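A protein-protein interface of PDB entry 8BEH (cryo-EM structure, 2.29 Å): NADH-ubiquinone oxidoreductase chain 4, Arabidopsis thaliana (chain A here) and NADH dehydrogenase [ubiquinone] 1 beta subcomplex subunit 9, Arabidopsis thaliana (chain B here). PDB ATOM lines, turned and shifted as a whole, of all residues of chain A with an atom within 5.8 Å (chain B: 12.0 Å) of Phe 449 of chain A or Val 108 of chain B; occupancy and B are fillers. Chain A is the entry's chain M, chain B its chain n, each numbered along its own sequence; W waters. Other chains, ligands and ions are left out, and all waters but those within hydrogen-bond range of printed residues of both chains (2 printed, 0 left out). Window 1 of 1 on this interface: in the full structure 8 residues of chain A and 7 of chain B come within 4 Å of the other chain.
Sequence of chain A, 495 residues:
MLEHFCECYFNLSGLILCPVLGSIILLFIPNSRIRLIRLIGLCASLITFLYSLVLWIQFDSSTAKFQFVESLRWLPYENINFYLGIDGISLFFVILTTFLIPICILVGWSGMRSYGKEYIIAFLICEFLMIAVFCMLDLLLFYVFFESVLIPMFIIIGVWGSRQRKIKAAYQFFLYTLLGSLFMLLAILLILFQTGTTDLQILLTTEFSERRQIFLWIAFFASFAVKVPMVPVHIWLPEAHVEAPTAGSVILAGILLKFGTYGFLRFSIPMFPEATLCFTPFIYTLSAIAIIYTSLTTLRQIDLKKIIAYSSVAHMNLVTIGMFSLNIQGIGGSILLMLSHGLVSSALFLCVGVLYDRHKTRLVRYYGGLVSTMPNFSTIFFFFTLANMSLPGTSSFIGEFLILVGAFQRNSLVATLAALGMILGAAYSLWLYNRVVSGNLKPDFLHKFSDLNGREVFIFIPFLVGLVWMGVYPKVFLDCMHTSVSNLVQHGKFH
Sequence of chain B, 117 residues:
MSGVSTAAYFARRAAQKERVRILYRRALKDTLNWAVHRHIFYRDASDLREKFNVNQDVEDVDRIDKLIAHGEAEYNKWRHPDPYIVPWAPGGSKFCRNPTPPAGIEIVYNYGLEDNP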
ATOM      1  N   HIS A 359      11.384  22.955  11.672  1.00  0.00           N
ATOM      2  CA  HIS A 359      12.015  22.789  12.996  1.00  0.00           C
ATOM      3  C   HIS A 359      12.548  24.061  13.644  1.00  0.00           C
ATOM      4  O   HIS A 359      12.842  23.962  14.787  1.00  0.00           O
ATOM      5  CB  HIS A 359      13.037  21.615  12.880  1.00  0.00           C
ATOM      6  CG  HIS A 359      12.410  20.412  12.273  1.00  0.00           C
ATOM      7  ND1 HIS A 359      11.284  19.840  12.798  1.00  0.00           N
ATOM      8  CD2 HIS A 359      12.716  19.702  11.170  1.00  0.00           C
ATOM      9  CE1 HIS A 359      10.935  18.812  12.073  1.00  0.00           C
ATOM     10  NE2 HIS A 359      11.796  18.702  11.079  1.00  0.00           N
ATOM     11  N   LEU A 370      17.856  11.863  10.037  1.00  0.00           N
ATOM     12  CA  LEU A 370      16.747  12.280   9.188  1.00  0.00           C
ATOM     13  C   LEU A 370      16.523  11.361   7.990  1.00  0.00           C
ATOM     14  O   LEU A 370      15.472  11.461   7.352  1.00  0.00           O
ATOM     15  CB  LEU A 370      16.975  13.713   8.702  1.00  0.00           C
ATOM     16  CG  LEU A 370      16.716  14.849   9.700  1.00  0.00           C
ATOM     17  CD1 LEU A 370      16.920  16.208   9.041  1.00  0.00           C
ATOM     18  CD2 LEU A 370      15.331  14.749  10.320  1.00  0.00           C
ATOM     19  N   THR A 373      13.260   9.425   8.515  1.00  0.00           N
ATOM     20  CA  THR A 373      11.974  10.107   8.477  1.00  0.00           C
ATOM     21  C   THR A 373      11.762  10.946   7.226  1.00  0.00           C
ATOM     22  O   THR A 373      10.609  11.182   6.860  1.00  0.00           O
ATOM     23  CB  THR A 373      11.779  11.008   9.711  1.00  0.00           C
ATOM     24  OG1 THR A 373      12.832  11.975   9.800  1.00  0.00           O
ATOM     25  CG2 THR A 373      11.743  10.175  10.985  1.00  0.00           C
ATOM     26  N   MET A 374      12.828  11.396   6.565  1.00  0.00           N
ATOM     27  CA  MET A 374      12.721  12.223   5.359  1.00  0.00           C
ATOM     28  C   MET A 374      13.629  11.687   4.256  1.00  0.00           C
ATOM     29  O   MET A 374      14.557  12.368   3.812  1.00  0.00           O
ATOM     30  CB  MET A 374      13.056  13.680   5.680  1.00  0.00           C
ATOM     31  CG  MET A 374      12.400  14.236   6.940  1.00  0.00           C
ATOM     32  SD  MET A 374      12.987  15.880   7.413  1.00  0.00           S
ATOM     33  CE  MET A 374      12.572  16.860   5.978  1.00  0.00           C
ATOM     34  N   LEU A 441      17.930   9.170  15.213  1.00  0.00           N
ATOM     35  CA  LEU A 441      17.109  10.290  15.627  1.00  0.00           C
ATOM     36  C   LEU A 441      17.385  10.635  17.087  1.00  0.00           C
ATOM     37  O   LEU A 441      17.873   9.818  17.870  1.00  0.00           O
ATOM     38  CB  LEU A 441      15.628   9.978  15.434  1.00  0.00           C
ATOM     39  CG  LEU A 441      15.163   9.666  14.013  1.00  0.00           C
ATOM     40  CD1 LEU A 441      13.896   8.824  14.052  1.00  0.00           C
ATOM     41  CD2 LEU A 441      14.962  10.941  13.210  1.00  0.00           C
ATOM     42  N   LEU A 446      13.691  16.494  18.446  1.00  0.00           N
ATOM     43  CA  LEU A 446      12.757  16.461  17.327  1.00  0.00           C
ATOM     44  C   LEU A 446      12.106  15.080  17.301  1.00  0.00           C
ATOM     45  O   LEU A 446      12.821  14.111  17.315  1.00  0.00           O
ATOM     46  CB  LEU A 446      13.536  16.798  16.042  1.00  0.00           C
ATOM     47  CG  LEU A 446      14.058  18.224  15.892  1.00  0.00           C
ATOM     48  CD1 LEU A 446      15.023  18.332  14.724  1.00  0.00           C
ATOM     49  CD2 LEU A 446      12.915  19.203  15.733  1.00  0.00           C
ATOM     50  N   HIS A 447      10.811  15.019  17.164  1.00  0.00           N
ATOM     51  CA  HIS A 447      10.057  13.750  17.227  1.00  0.00           C
ATOM     52  C   HIS A 447       8.950  13.768  16.178  1.00  0.00           C
ATOM     53  O   HIS A 447       8.396  12.748  15.923  1.00  0.00           O
ATOM     54  CB  HIS A 447       9.597  13.489  18.672  1.00  0.00           C
ATOM     55  CG  HIS A 447       8.543  14.451  19.070  1.00  0.00           C
ATOM     56  ND1 HIS A 447       8.769  15.796  19.091  1.00  0.00           N
ATOM     57  CD2 HIS A 447       7.247  14.289  19.358  1.00  0.00           C
ATOM     58  CE1 HIS A 447       7.681  16.429  19.439  1.00  0.00           C
ATOM     59  NE2 HIS A 447       6.753  15.532  19.622  1.00  0.00           N
ATOM     60  N   LYS A 448       8.670  14.911  15.615  1.00  0.00           N
ATOM     61  CA  LYS A 448       7.635  15.055  14.573  1.00  0.00           C
ATOM     62  C   LYS A 448       8.279  15.497  13.244  1.00  0.00           C
ATOM     63  O   LYS A 448       8.988  16.433  13.229  1.00  0.00           O
ATOM     64  CB  LYS A 448       6.478  15.879  15.137  1.00  0.00           C
ATOM     65  CG  LYS A 448       5.349  16.257  14.214  1.00  0.00           C
ATOM     66  CD  LYS A 448       4.306  17.076  14.944  1.00  0.00           C
ATOM     67  CE  LYS A 448       3.651  16.310  16.066  1.00  0.00           C
ATOM     68  NZ  LYS A 448       2.686  15.319  15.534  1.00  0.00           N
ATOM     69  N   PHE A 449       7.947  14.811  12.169  1.00  0.00           N
ATOM     70  CA  PHE A 449       8.645  15.016  10.878  1.00  0.00           C
ATOM     71  C   PHE A 449       7.685  14.981   9.696  1.00  0.00           C
ATOM     72  O   PHE A 449       6.657  14.402   9.743  1.00  0.00           O
ATOM     73  CB  PHE A 449       9.862  14.061  10.706  1.00  0.00           C
ATOM     74  CG  PHE A 449      10.833  13.984  11.845  1.00  0.00           C
ATOM     75  CD1 PHE A 449      10.604  13.131  12.909  1.00  0.00           C
ATOM     76  CD2 PHE A 449      11.988  14.744  11.829  1.00  0.00           C
ATOM     77  CE1 PHE A 449      11.504  13.065  13.955  1.00  0.00           C
ATOM     78  CE2 PHE A 449      12.886  14.669  12.874  1.00  0.00           C
ATOM     79  CZ  PHE A 449      12.643  13.832  13.932  1.00  0.00           C
ATOM     80  N   SER A 450       8.091  15.637   8.637  1.00  0.00           N
ATOM     81  CA  SER A 450       7.376  15.607   7.370  1.00  0.00           C
ATOM     82  C   SER A 450       8.386  15.698   6.239  1.00  0.00           C
ATOM     83  O   SER A 450       9.215  16.610   6.223  1.00  0.00           O
ATOM     84  CB  SER A 450       6.367  16.756   7.268  1.00  0.00           C
ATOM     85  OG  SER A 450       5.436  16.515   6.237  1.00  0.00           O
ATOM     86  N   ASP A 451       8.312  14.758   5.299  1.00  0.00           N
ATOM     87  CA  ASP A 451       9.133  14.832   4.100  1.00  0.00           C
ATOM     88  C   ASP A 451       8.602  15.934   3.181  1.00  0.00           C
ATOM     89  O   ASP A 451       7.648  16.645   3.499  1.00  0.00           O
ATOM     90  CB  ASP A 451       9.170  13.477   3.392  1.00  0.00           C
ATOM     91  CG  ASP A 451      10.542  13.159   2.793  1.00  0.00           C
ATOM     92  OD1 ASP A 451      11.350  14.084   2.590  1.00  0.00           O
ATOM     93  OD2 ASP A 451      10.807  11.976   2.512  1.00  0.00           O
ATOM     94  N   PRO B 101      13.524   1.003  16.022  1.00  0.00           N
ATOM     95  CA  PRO B 101      13.292   2.439  15.962  1.00  0.00           C
ATOM     96  C   PRO B 101      12.884   2.975  17.318  1.00  0.00           C
ATOM     97  O   PRO B 101      12.266   2.260  18.130  1.00  0.00           O
ATOM     98  CB  PRO B 101      12.153   2.572  14.940  1.00  0.00           C
ATOM     99  CG  PRO B 101      12.073   1.276  14.245  1.00  0.00           C
ATOM    100  CD  PRO B 101      12.601   0.240  15.167  1.00  0.00           C
ATOM    101  N   PRO B 102      13.213   4.227  17.613  1.00  0.00           N
ATOM    102  CA  PRO B 102      12.727   4.843  18.851  1.00  0.00           C
ATOM    103  C   PRO B 102      11.216   4.996  18.830  1.00  0.00           C
ATOM    104  O   PRO B 102      10.591   5.120  17.774  1.00  0.00           O
ATOM    105  CB  PRO B 102      13.421   6.208  18.877  1.00  0.00           C
ATOM    106  CG  PRO B 102      13.827   6.475  17.468  1.00  0.00           C
ATOM    107  CD  PRO B 102      13.981   5.159  16.769  1.00  0.00           C
ATOM    108  N   ALA B 103      10.629   4.970  20.020  1.00  0.00           N
ATOM    109  CA  ALA B 103       9.217   5.271  20.170  1.00  0.00           C
ATOM    110  C   ALA B 103       9.008   6.778  20.295  1.00  0.00           C
ATOM    111  O   ALA B 103       9.922   7.534  20.636  1.00  0.00           O
ATOM    112  CB  ALA B 103       8.637   4.557  21.388  1.00  0.00           C
ATOM    113  N   GLY B 104       7.783   7.210  20.014  1.00  0.00           N
ATOM    114  CA  GLY B 104       7.441   8.614  20.094  1.00  0.00           C
ATOM    115  C   GLY B 104       7.657   9.413  18.831  1.00  0.00           C
ATOM    116  O   GLY B 104       7.705  10.645  18.897  1.00  0.00           O
ATOM    117  N   ILE B 105       7.785   8.758  17.683  1.00  0.00           N
ATOM    118  CA  ILE B 105       8.025   9.430  16.414  1.00  0.00           C
ATOM    119  C   ILE B 105       6.701   9.533  15.679  1.00  0.00           C
ATOM    120  O   ILE B 105       6.006   8.529  15.493  1.00  0.00           O
ATOM    121  CB  ILE B 105       9.065   8.673  15.569  1.00  0.00           C
ATOM    122  CG1 ILE B 105      10.422   8.648  16.276  1.00  0.00           C
ATOM    123  CG2 ILE B 105       9.184   9.296  14.183  1.00  0.00           C
ATOM    124  CD1 ILE B 105      10.864   9.981  16.834  1.00  0.00           C
ATOM    125  N   GLU B 106       6.347  10.760  15.325  1.00  0.00           N
ATOM    126  CA  GLU B 106       5.115  11.047  14.560  1.00  0.00           C
ATOM    127  C   GLU B 106       5.454  11.542  13.137  1.00  0.00           C
ATOM    128  O   GLU B 106       6.381  12.319  13.005  1.00  0.00           O
ATOM    129  CB  GLU B 106       4.283  12.016  15.385  1.00  0.00           C
ATOM    130  CG  GLU B 106       3.939  11.487  16.749  1.00  0.00           C
ATOM    131  CD  GLU B 106       3.674  12.538  17.805  1.00  0.00           C
ATOM    132  OE1 GLU B 106       2.945  13.483  17.511  1.00  0.00           O
ATOM    133  OE2 GLU B 106       4.189  12.384  18.932  1.00  0.00           O
ATOM    134  N   ILE B 107       4.764  11.089  12.121  1.00  0.00           N
ATOM    135  CA  ILE B 107       4.954  11.546  10.751  1.00  0.00           C
ATOM    136  C   ILE B 107       3.746  12.387  10.374  1.00  0.00           C
ATOM    137  O   ILE B 107       2.603  11.945  10.542  1.00  0.00           O
ATOM    138  CB  ILE B 107       5.123  10.358   9.785  1.00  0.00           C
ATOM    139  CG1 ILE B 107       6.344   9.508  10.158  1.00  0.00           C
ATOM    140  CG2 ILE B 107       5.229  10.843   8.353  1.00  0.00           C
ATOM    141  CD1 ILE B 107       7.640  10.265  10.274  1.00  0.00           C
ATOM    142  N   VAL B 108       3.959  13.580   9.877  1.00  0.00           N
ATOM    143  CA  VAL B 108       2.834  14.516   9.572  1.00  0.00           C
ATOM    144  C   VAL B 108       2.572  14.480   8.076  1.00  0.00           C
ATOM    145  O   VAL B 108       3.507  14.462   7.275  1.00  0.00           O
ATOM    146  CB  VAL B 108       3.074  15.977  10.048  1.00  0.00           C
ATOM    147  CG1 VAL B 108       1.913  16.921   9.851  1.00  0.00           C
ATOM    148  CG2 VAL B 108       3.705  16.098  11.407  1.00  0.00           C
ATOM    149  N   TYR B 109       1.330  14.525   7.739  1.00  0.00           N
ATOM    150  CA  TYR B 109       0.842  14.535   6.372  1.00  0.00           C
ATOM    151  C   TYR B 109       0.253  15.902   6.052  1.00  0.00           C
ATOM    152  O   TYR B 109      -0.166  16.638   6.949  1.00  0.00           O
ATOM    153  CB  TYR B 109      -0.216  13.446   6.169  1.00  0.00           C
ATOM    154  CG  TYR B 109       0.346  12.048   6.151  1.00  0.00           C
ATOM    155  CD1 TYR B 109       1.654  11.806   5.754  1.00  0.00           C
ATOM    156  CD2 TYR B 109      -0.418  10.973   6.577  1.00  0.00           C
ATOM    157  CE1 TYR B 109       2.169  10.527   5.747  1.00  0.00           C
ATOM    158  CE2 TYR B 109       0.086   9.697   6.579  1.00  0.00           C
ATOM    159  CZ  TYR B 109       1.381   9.478   6.165  1.00  0.00           C
ATOM    160  OH  TYR B 109       1.881   8.201   6.167  1.00  0.00           O
ATOM    161  N   ASN B 110       0.248  16.240   4.761  1.00  0.00           N
ATOM    162  CA  ASN B 110      -0.380  17.461   4.251  1.00  0.00           C
ATOM    163  C   ASN B 110       0.225  18.718   4.877  1.00  0.00           C
ATOM    164  O   ASN B 110      -0.478  19.651   5.266  1.00  0.00           O
ATOM    165  CB  ASN B 110      -1.897  17.418   4.457  1.00  0.00           C
ATOM    166  CG  ASN B 110      -2.502  16.097   4.032  1.00  0.00           C
ATOM    167  OD1 ASN B 110      -2.312  15.650   2.904  1.00  0.00           O
ATOM    168  ND2 ASN B 110      -3.224  15.460   4.937  1.00  0.00           N
ATOM    169  N   TYR B 111       1.548  18.741   4.960  1.00  0.00           N
ATOM    170  CA  TYR B 111       2.278  19.900   5.443  1.00  0.00           C
ATOM    171  C   TYR B 111       2.486  20.917   4.325  1.00  0.00           C
ATOM    172  O   TYR B 111       2.587  20.568   3.148  1.00  0.00           O
ATOM    173  CB  TYR B 111       3.630  19.477   6.018  1.00  0.00           C
ATOM    174  CG  TYR B 111       4.440  20.617   6.589  1.00  0.00           C
ATOM    175  CD1 TYR B 111       4.122  21.174   7.820  1.00  0.00           C
ATOM    176  CD2 TYR B 111       5.516  21.144   5.888  1.00  0.00           C
ATOM    177  CE1 TYR B 111       4.855  22.216   8.340  1.00  0.00           C
ATOM    178  CE2 TYR B 111       6.253  22.186   6.399  1.00  0.00           C
ATOM    179  CZ  TYR B 111       5.918  22.720   7.628  1.00  0.00           C
ATOM    180  OH  TYR B 111       6.650  23.763   8.144  1.00  0.00           O
ATOM    181  N   GLY B 112       2.541  22.188   4.712  1.00  0.00           N
ATOM    182  CA  GLY B 112       2.883  23.256   3.792  1.00  0.00           C
ATOM    183  C   GLY B 112       1.894  23.519   2.677  1.00  0.00           C
ATOM    184  O   GLY B 112       2.303  23.914   1.585  1.00  0.00           O
ATOM    185  N   LEU B 113       0.604  23.317   2.924  1.00  0.00           N
ATOM    186  CA  LEU B 113      -0.409  23.593   1.917  1.00  0.00           C
ATOM    187  C   LEU B 113      -0.571  25.097   1.718  1.00  0.00           C
ATOM    188  O   LEU B 113      -0.298  25.897   2.615  1.00  0.00           O
ATOM    189  CB  LEU B 113      -1.741  22.965   2.322  1.00  0.00           C
ATOM    190  CG  LEU B 113      -1.683  21.445   2.494  1.00  0.00           C
ATOM    191  CD1 LEU B 113      -2.944  20.905   3.137  1.00  0.00           C
ATOM    192  CD2 LEU B 113      -1.442  20.787   1.153  1.00  0.00           C
HETATM  193  O   HOH W   1       4.341  14.868  19.719  1.00  0.00           O
HETATM  194  O   HOH W   2       1.964  13.896  12.525  1.00  0.00           O
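The backbone carbonyl oxygen (O) of Val 108 of chain B is in hydrogen-bond range of the side-chain hydroxyl (OG) of Ser 450 of chain A (3.0 Å). The backbone NH (N) of Glu 106 of chain B lies within hydrogen-bond range of the backbone carbonyl oxygen (O) of His 447 of chain A, at 2.9 Å. The side-chain amino group of Lys 448 of chain A lies within salt-bridge range of the side-chain carboxylate of Glu 106 of chain B. The backbone NH (N) of Val 108 of chain B lies within hydrogen-bond range of the backbone carbonyl oxygen (O) of Phe 449 of chain A, 2.8 Å away. The backbone carbonyl oxygen (O) of Glu 106 of chain B sits at hydrogen-bond distance from the backbone NH (N) of Phe 449 of chain A (3.1 Å).
Water W1 lies within hydrogen-bond range of NE2 of His 447 of chain A (2.5 Å) and OE2 of Glu 106 of chain B (2.6 Å). Water W2 lies within hydrogen-bond range of the backbone carbonyl oxygen of Ile 107 of chain B (2.9 Å), the backbone NH of Val 108 of chain B (3.3 Å) and the side-chain amino group of Lys 448 of chain A (3.4 Å).
Hydrophobic or aromatic side chains of chain A that line the printed part of chain B: His 447. Of the 13 printed residues of chain B, 6 touch a printed residue of chain A. Along chain B the printed residues that touch a printed residue of chain A span positions 104 to 111.
Among the printed residues, merely in contact across the chains: Lys 448 of chain A with Val 108 of chain B (3.3 Å), His 447 of chain A with Ile 105 of chain B (3.4 Å), His 447 of chain A with Gly 104 of chain B (3.4 Å), Phe 449 of chain A with Ile 107 of chain B (3.5 Å) and Ser 450 of chain A with Tyr 111 of chain B (3.5 Å).
Phe 449 of chain A touches just these residues of chain B: Glu 106, Ile 107 and Val 108. Val 108 of chain B touches three residues of chain A. No residue of chain B comes within 4 Å of Thr 373 of chain A. No residue of chain B comes within 4 Å of Leu 441 of chain A. Leu 446 of chain A touches none of the printed residues of chain B. Of chain B, only Glu 106 and Val 108 come within 4 Å of Lys 448 of chain A. Printed residues of chain A within 4 Å of Tyr 111 of chain B: Ser 450. Printed residues of chain A within 4 Å of Ile 105 of chain B: His 447. Of the printed residues of chain A, Ile 107 of chain B touches Phe 449 (3.5 Å). Pro 102 of chain B touches none of the printed residues of chain A. The nearest residue of chain B that does not touch Phe 449 of chain A is Ile 105 of chain B (4.3 Å). The nearest printed residue of chain A that does not touch Ile 105 of chain B is Leu 441 of chain A (4.1 Å).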
